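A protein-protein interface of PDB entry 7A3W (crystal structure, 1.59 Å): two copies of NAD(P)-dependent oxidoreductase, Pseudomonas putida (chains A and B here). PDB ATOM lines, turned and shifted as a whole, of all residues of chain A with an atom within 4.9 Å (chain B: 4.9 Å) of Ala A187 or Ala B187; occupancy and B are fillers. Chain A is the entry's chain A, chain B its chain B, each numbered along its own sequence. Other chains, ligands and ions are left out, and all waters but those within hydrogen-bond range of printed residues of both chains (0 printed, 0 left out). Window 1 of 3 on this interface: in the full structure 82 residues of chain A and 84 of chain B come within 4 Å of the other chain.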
ATOM      1  N   ALA A 182      16.329   2.444  -7.653  1.00  0.00           N
ATOM      2  CA  ALA A 182      16.564   1.457  -6.575  1.00  0.00           C
ATOM      3  C   ALA A 182      15.256   0.708  -6.334  1.00  0.00           C
ATOM      4  O   ALA A 182      15.249  -0.526  -6.318  1.00  0.00           O
ATOM      5  CB  ALA A 182      17.063   2.114  -5.321  1.00  0.00           C
ATOM      6  N   PHE A 183      14.157   1.457  -6.228  1.00  0.00           N
ATOM      7  CA  PHE A 183      12.809   0.908  -6.062  1.00  0.00           C
ATOM      8  C   PHE A 183      12.473   0.066  -7.288  1.00  0.00           C
ATOM      9  O   PHE A 183      12.110  -1.122  -7.138  1.00  0.00           O
ATOM     10  CB  PHE A 183      11.825   2.059  -5.838  1.00  0.00           C
ATOM     11  CG  PHE A 183      10.381   1.697  -6.002  1.00  0.00           C
ATOM     12  CD1 PHE A 183       9.874   0.475  -5.567  1.00  0.00           C
ATOM     13  CD2 PHE A 183       9.517   2.577  -6.624  1.00  0.00           C
ATOM     14  CE1 PHE A 183       8.539   0.159  -5.744  1.00  0.00           C
ATOM     15  CE2 PHE A 183       8.191   2.235  -6.826  1.00  0.00           C
ATOM     16  CZ  PHE A 183       7.697   1.038  -6.371  1.00  0.00           C
ATOM     17  N   TYR A 184      12.554   0.661  -8.486  1.00  0.00           N
ATOM     18  CA  TYR A 184      12.064  -0.023  -9.705  1.00  0.00           C
ATOM     19  C   TYR A 184      12.782  -1.360  -9.918  1.00  0.00           C
ATOM     20  O   TYR A 184      12.091  -2.386 -10.094  1.00  0.00           O
ATOM     21  CB  TYR A 184      12.210   0.832 -10.955  1.00  0.00           C
ATOM     22  CG  TYR A 184      11.706   0.104 -12.173  1.00  0.00           C
ATOM     23  CD1 TYR A 184      12.528  -0.707 -12.926  1.00  0.00           C
ATOM     24  CD2 TYR A 184      10.385   0.195 -12.558  1.00  0.00           C
ATOM     25  CE1 TYR A 184      12.063  -1.397 -14.037  1.00  0.00           C
ATOM     26  CE2 TYR A 184       9.909  -0.461 -13.673  1.00  0.00           C
ATOM     27  CZ  TYR A 184      10.744  -1.255 -14.428  1.00  0.00           C
ATOM     28  OH  TYR A 184      10.296  -1.963 -15.496  1.00  0.00           O
ATOM     29  N   PHE A 185      14.109  -1.407  -9.853  1.00  0.00           N
ATOM     30  CA  PHE A 185      14.823  -2.659 -10.219  1.00  0.00           C
ATOM     31  C   PHE A 185      14.801  -3.674  -9.067  1.00  0.00           C
ATOM     32  O   PHE A 185      14.747  -4.899  -9.362  1.00  0.00           O
ATOM     33  CB  PHE A 185      16.206  -2.408 -10.810  1.00  0.00           C
ATOM     34  CG  PHE A 185      16.090  -1.964 -12.245  1.00  0.00           C
ATOM     35  CD1 PHE A 185      15.478  -2.781 -13.181  1.00  0.00           C
ATOM     36  CD2 PHE A 185      16.475  -0.691 -12.629  1.00  0.00           C
ATOM     37  CE1 PHE A 185      15.258  -2.359 -14.480  1.00  0.00           C
ATOM     38  CE2 PHE A 185      16.275  -0.275 -13.934  1.00  0.00           C
ATOM     39  CZ  PHE A 185      15.685  -1.117 -14.858  1.00  0.00           C
ATOM     40  N   GLY A 186      14.805  -3.214  -7.822  1.00  0.00           N
ATOM     41  CA  GLY A 186      14.554  -4.144  -6.696  1.00  0.00           C
ATOM     42  C   GLY A 186      13.196  -4.808  -6.851  1.00  0.00           C
ATOM     43  O   GLY A 186      13.064  -6.019  -6.613  1.00  0.00           O
ATOM     44  N   ALA A 187      12.182  -4.021  -7.221  1.00  0.00           N
ATOM     45  CA  ALA A 187      10.835  -4.531  -7.469  1.00  0.00           C
ATOM     46  C   ALA A 187      10.791  -5.480  -8.676  1.00  0.00           C
ATOM     47  O   ALA A 187      10.050  -6.482  -8.642  1.00  0.00           O
ATOM     48  CB  ALA A 187       9.884  -3.370  -7.629  1.00  0.00           C
ATOM     49  N   PHE A 188      11.534  -5.165  -9.733  1.00  0.00           N
ATOM     50  CA  PHE A 188      11.534  -5.971 -10.973  1.00  0.00           C
ATOM     51  C   PHE A 188      12.211  -7.298 -10.672  1.00  0.00           C
ATOM     52  O   PHE A 188      11.678  -8.333 -11.098  1.00  0.00           O
ATOM     53  CB  PHE A 188      12.193  -5.240 -12.145  1.00  0.00           C
ATOM     54  CG  PHE A 188      12.045  -5.980 -13.442  1.00  0.00           C
ATOM     55  CD1 PHE A 188      10.820  -6.046 -14.095  1.00  0.00           C
ATOM     56  CD2 PHE A 188      13.114  -6.647 -14.001  1.00  0.00           C
ATOM     57  CE1 PHE A 188      10.675  -6.752 -15.272  1.00  0.00           C
ATOM     58  CE2 PHE A 188      12.959  -7.350 -15.182  1.00  0.00           C
ATOM     59  CZ  PHE A 188      11.741  -7.414 -15.813  1.00  0.00           C
ATOM     60  N   ALA A 189      13.287  -7.291  -9.892  1.00  0.00           N
ATOM     61  CA  ALA A 189      13.945  -8.556  -9.485  1.00  0.00           C
ATOM     62  C   ALA A 189      12.977  -9.394  -8.633  1.00  0.00           C
ATOM     63  O   ALA A 189      12.911 -10.624  -8.800  1.00  0.00           O
ATOM     64  CB  ALA A 189      15.227  -8.302  -8.741  1.00  0.00           C
ATOM     65  N   ALA A 190      12.222  -8.754  -7.732  1.00  0.00           N
ATOM     66  CA  ALA A 190      11.215  -9.447  -6.903  1.00  0.00           C
ATOM     67  C   ALA A 190      10.196 -10.086  -7.842  1.00  0.00           C
ATOM     68  O   ALA A 190       9.799 -11.222  -7.591  1.00  0.00           O
ATOM     69  CB  ALA A 190      10.547  -8.493  -5.933  1.00  0.00           C
ATOM     70  N   TRP A 191       9.723  -9.350  -8.857  1.00  0.00           N
ATOM     71  CA  TRP A 191       8.729  -9.910  -9.806  1.00  0.00           C
ATOM     72  C   TRP A 191       9.301 -11.170 -10.484  1.00  0.00           C
ATOM     73  O   TRP A 191       8.599 -12.202 -10.556  1.00  0.00           O
ATOM     74  CB  TRP A 191       8.304  -8.887 -10.842  1.00  0.00           C
ATOM     75  CG  TRP A 191       7.260  -9.474 -11.739  1.00  0.00           C
ATOM     76  CD1 TRP A 191       5.927  -9.570 -11.480  1.00  0.00           C
ATOM     77  CD2 TRP A 191       7.472 -10.123 -12.999  1.00  0.00           C
ATOM     78  NE1 TRP A 191       5.283 -10.166 -12.531  1.00  0.00           N
ATOM     79  CE2 TRP A 191       6.207 -10.549 -13.460  1.00  0.00           C
ATOM     80  CE3 TRP A 191       8.586 -10.331 -13.815  1.00  0.00           C
ATOM     81  CZ2 TRP A 191       6.039 -11.215 -14.672  1.00  0.00           C
ATOM     82  CZ3 TRP A 191       8.424 -11.011 -15.001  1.00  0.00           C
ATOM     83  CH2 TRP A 191       7.165 -11.414 -15.440  1.00  0.00           C
ATOM     84  N   LEU A 219       0.440  -2.724  -3.908  1.00  0.00           N
ATOM     85  CA  LEU A 219       1.700  -1.989  -3.631  1.00  0.00           C
ATOM     86  C   LEU A 219       1.476  -0.475  -3.784  1.00  0.00           C
ATOM     87  O   LEU A 219       1.987   0.293  -3.004  1.00  0.00           O
ATOM     88  CB  LEU A 219       2.796  -2.500  -4.569  1.00  0.00           C
ATOM     89  CG  LEU A 219       4.177  -1.880  -4.349  1.00  0.00           C
ATOM     90  CD1 LEU A 219       4.712  -2.159  -2.946  1.00  0.00           C
ATOM     91  CD2 LEU A 219       5.158  -2.378  -5.397  1.00  0.00           C
ATOM     92  N   ALA B 182       6.025 -13.152  -2.803  1.00  0.00           N
ATOM     93  CA  ALA B 182       7.480 -13.011  -3.031  1.00  0.00           C
ATOM     94  C   ALA B 182       7.721 -11.711  -3.811  1.00  0.00           C
ATOM     95  O   ALA B 182       8.564 -10.903  -3.412  1.00  0.00           O
ATOM     96  CB  ALA B 182       8.021 -14.212  -3.742  1.00  0.00           C
ATOM     97  N   PHE B 183       6.918 -11.476  -4.851  1.00  0.00           N
ATOM     98  CA  PHE B 183       6.944 -10.246  -5.653  1.00  0.00           C
ATOM     99  C   PHE B 183       6.616  -9.058  -4.749  1.00  0.00           C
ATOM    100  O   PHE B 183       7.361  -8.089  -4.695  1.00  0.00           O
ATOM    101  CB  PHE B 183       5.962 -10.395  -6.816  1.00  0.00           C
ATOM    102  CG  PHE B 183       5.612  -9.118  -7.529  1.00  0.00           C
ATOM    103  CD1 PHE B 183       6.570  -8.146  -7.770  1.00  0.00           C
ATOM    104  CD2 PHE B 183       4.303  -8.854  -7.905  1.00  0.00           C
ATOM    105  CE1 PHE B 183       6.244  -6.956  -8.411  1.00  0.00           C
ATOM    106  CE2 PHE B 183       3.981  -7.679  -8.559  1.00  0.00           C
ATOM    107  CZ  PHE B 183       4.937  -6.711  -8.783  1.00  0.00           C
ATOM    108  N   TYR B 184       5.476  -9.116  -4.059  1.00  0.00           N
ATOM    109  CA  TYR B 184       4.968  -7.956  -3.283  1.00  0.00           C
ATOM    110  C   TYR B 184       5.992  -7.488  -2.252  1.00  0.00           C
ATOM    111  O   TYR B 184       6.320  -6.289  -2.241  1.00  0.00           O
ATOM    112  CB  TYR B 184       3.653  -8.234  -2.569  1.00  0.00           C
ATOM    113  CG  TYR B 184       3.174  -7.007  -1.839  1.00  0.00           C
ATOM    114  CD1 TYR B 184       2.373  -6.081  -2.467  1.00  0.00           C
ATOM    115  CD2 TYR B 184       3.525  -6.781  -0.517  1.00  0.00           C
ATOM    116  CE1 TYR B 184       1.923  -4.954  -1.802  1.00  0.00           C
ATOM    117  CE2 TYR B 184       3.079  -5.659   0.168  1.00  0.00           C
ATOM    118  CZ  TYR B 184       2.255  -4.751  -0.479  1.00  0.00           C
ATOM    119  OH  TYR B 184       1.835  -3.602   0.123  1.00  0.00           O
ATOM    120  N   PHE B 185       6.537  -8.394  -1.436  1.00  0.00           N
ATOM    121  CA  PHE B 185       7.394  -7.968  -0.304  1.00  0.00           C
ATOM    122  C   PHE B 185       8.819  -7.675  -0.787  1.00  0.00           C
ATOM    123  O   PHE B 185       9.458  -6.739  -0.221  1.00  0.00           O
ATOM    124  CB  PHE B 185       7.290  -8.920   0.883  1.00  0.00           C
ATOM    125  CG  PHE B 185       6.031  -8.659   1.661  1.00  0.00           C
ATOM    126  CD1 PHE B 185       5.781  -7.401   2.205  1.00  0.00           C
ATOM    127  CD2 PHE B 185       5.058  -9.635   1.768  1.00  0.00           C
ATOM    128  CE1 PHE B 185       4.595  -7.127   2.860  1.00  0.00           C
ATOM    129  CE2 PHE B 185       3.863  -9.355   2.423  1.00  0.00           C
ATOM    130  CZ  PHE B 185       3.633  -8.106   2.964  1.00  0.00           C
ATOM    131  N   GLY B 186       9.309  -8.379  -1.804  1.00  0.00           N
ATOM    132  CA  GLY B 186      10.568  -7.980  -2.454  1.00  0.00           C
ATOM    133  C   GLY B 186      10.470  -6.564  -2.997  1.00  0.00           C
ATOM    134  O   GLY B 186      11.416  -5.780  -2.818  1.00  0.00           O
ATOM    135  N   ALA B 187       9.329  -6.226  -3.613  1.00  0.00           N
ATOM    136  CA  ALA B 187       9.069  -4.891  -4.173  1.00  0.00           C
ATOM    137  C   ALA B 187       8.910  -3.853  -3.057  1.00  0.00           C
ATOM    138  O   ALA B 187       9.363  -2.722  -3.230  1.00  0.00           O
ATOM    139  CB  ALA B 187       7.858  -4.942  -5.075  1.00  0.00           C
ATOM    140  N   PHE B 188       8.268  -4.216  -1.959  1.00  0.00           N
ATOM    141  CA  PHE B 188       8.033  -3.294  -0.832  1.00  0.00           C
ATOM    142  C   PHE B 188       9.381  -2.988  -0.179  1.00  0.00           C
ATOM    143  O   PHE B 188       9.637  -1.818   0.128  1.00  0.00           O
ATOM    144  CB  PHE B 188       7.036  -3.854   0.179  1.00  0.00           C
ATOM    145  CG  PHE B 188       6.692  -2.871   1.269  1.00  0.00           C
ATOM    146  CD1 PHE B 188       5.873  -1.775   1.007  1.00  0.00           C
ATOM    147  CD2 PHE B 188       7.185  -3.041   2.551  1.00  0.00           C
ATOM    148  CE1 PHE B 188       5.559  -0.883   2.014  1.00  0.00           C
ATOM    149  CE2 PHE B 188       6.890  -2.120   3.552  1.00  0.00           C
ATOM    150  CZ  PHE B 188       6.056  -1.063   3.285  1.00  0.00           C
ATOM    151  N   ALA B 189      10.242  -3.993  -0.029  1.00  0.00           N
ATOM    152  CA  ALA B 189      11.590  -3.768   0.528  1.00  0.00           C
ATOM    153  C   ALA B 189      12.377  -2.832  -0.412  1.00  0.00           C
ATOM    154  O   ALA B 189      13.094  -1.920   0.088  1.00  0.00           O
ATOM    155  CB  ALA B 189      12.296  -5.061   0.743  1.00  0.00           C
ATOM    156  N   ALA B 190      12.263  -3.039  -1.720  1.00  0.00           N
ATOM    157  CA  ALA B 190      12.918  -2.166  -2.726  1.00  0.00           C
ATOM    158  C   ALA B 190      12.408  -0.738  -2.527  1.00  0.00           C
ATOM    159  O   ALA B 190      13.196   0.187  -2.619  1.00  0.00           O
ATOM    160  CB  ALA B 190      12.626  -2.647  -4.138  1.00  0.00           C
ATOM    161  N   TRP B 191      11.093  -0.557  -2.357  1.00  0.00           N
ATOM    162  CA  TRP B 191      10.518   0.796  -2.174  1.00  0.00           C
ATOM    163  C   TRP B 191      11.137   1.465  -0.937  1.00  0.00           C
ATOM    164  O   TRP B 191      11.556   2.644  -1.023  1.00  0.00           O
ATOM    165  CB  TRP B 191       8.995   0.752  -2.077  1.00  0.00           C
ATOM    166  CG  TRP B 191       8.463   2.136  -1.915  1.00  0.00           C
ATOM    167  CD1 TRP B 191       8.229   3.034  -2.909  1.00  0.00           C
ATOM    168  CD2 TRP B 191       8.175   2.817  -0.678  1.00  0.00           C
ATOM    169  NE1 TRP B 191       7.776   4.213  -2.386  1.00  0.00           N
ATOM    170  CE2 TRP B 191       7.753   4.117  -1.019  1.00  0.00           C
ATOM    171  CE3 TRP B 191       8.201   2.453   0.671  1.00  0.00           C
ATOM    172  CZ2 TRP B 191       7.374   5.054  -0.057  1.00  0.00           C
ATOM    173  CZ3 TRP B 191       7.863   3.386   1.621  1.00  0.00           C
ATOM    174  CH2 TRP B 191       7.432   4.663   1.264  1.00  0.00           C
ATOM    175  N   LEU B 219       6.585  -0.094 -13.803  1.00  0.00           N
ATOM    176  CA  LEU B 219       6.670  -1.527 -13.422  1.00  0.00           C
ATOM    177  C   LEU B 219       5.455  -2.281 -13.980  1.00  0.00           C
ATOM    178  O   LEU B 219       5.609  -3.399 -14.483  1.00  0.00           O
ATOM    179  CB  LEU B 219       6.789  -1.657 -11.908  1.00  0.00           C
ATOM    180  CG  LEU B 219       6.937  -3.091 -11.390  1.00  0.00           C
ATOM    181  CD1 LEU B 219       8.236  -3.712 -11.893  1.00  0.00           C
ATOM    182  CD2 LEU B 219       6.918  -3.122  -9.865  1.00  0.00           C
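Of the 11 printed residues of chain B, 7 touch a printed residue of chain A. Hydrophobic or aromatic side chains of chain B that line the printed part of chain A: Phe B183, Tyr B184, Ala B187, Ala B190, Trp B191 and Leu B219. Of the 11 printed residues of chain A, 7 touch a printed residue of chain B. Printed residues of chain A that touch a printed residue of chain B: Phe A183, Tyr A184, Gly A186, Ala A187, Ala A190, Trp A191 and Leu A219. Hydrophobic or aromatic side chains of chain A within 4 Å of the printed part of chain B: Phe A183, Tyr A184, Ala A187, Ala A190, Trp A191 and Leu A219. Among the printed residues, 15 pairs touch across the chains.
Of the printed residues of chain B, Phe A183 touches Ala B187 (3.9 Å), Ala B190 (3.4 Å) and Trp B191 (3.5 Å). Ala A187 touches four residues of chain B. Printed residues of chain B within 4 Å of Leu A219: Tyr B184 (3.4 Å) and Ala B187 (3.7 Å). Printed residues of chain A within 4 Å of Tyr B184: Leu A219. Phe B185 touches none of the printed residues of chain A. Of chain A, only Phe A183 (3.9 Å), Ala A187 (3.6 Å), Ala A190 (3.5 Å) and Leu A219 (3.7 Å) come within 4 Å of Ala B187. The nearest residue of chain B that does not touch Ala A187 is Gly B186 (4.8 Å). The nearest residue of chain A that does not touch Ala B187 is Gly A186 (4.8 Å). The nearest printed residue of chain B that does not touch Ala A190 is Ala B182 (4.01 Å).
O of Ala B187 touches CE1 of Phe A183 (3.9 Å). CA of Trp B191 touches CD1 of Phe A183, at 3.5 Å. Tyr A184 touches Leu B219 (CE2 to N, 3.3 Å). Phe B183 touches Ala A187 (CE1 to O, 3.8 Å). Ala B187 touches Ala A187. N of Ala A187 touches CB of Ala B190, at 3.4 Å. CB of Ala A187 touches CD2 of Leu B219, at 3.7 Å. Ala A190 touches Ala B187. Trp A191 touches Phe B183 (CA to CD1, 3.5 Å). Leu A219 touches Ala B187 (CD2 to CB, 3.7 Å).
Phe A183 touches Ala B187, and with the chains exchanged Ala A187 touches Phe B183. Phe A183 touches Trp B191, and with the chains exchanged Trp A191 touches Phe B183. Tyr A184 touches Leu B219, and with the chains exchanged Leu A219 touches Tyr B184. Ala A187 touches its own counterpart, Ala B187. Positions printed for both chains: 182, 183, 184, 185, 186, 187, 188, 189, 190, 191 and 219. Of the 15 pairs that touch across the chains among the printed residues, 15 have their exchanged pair printed and touching as well.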
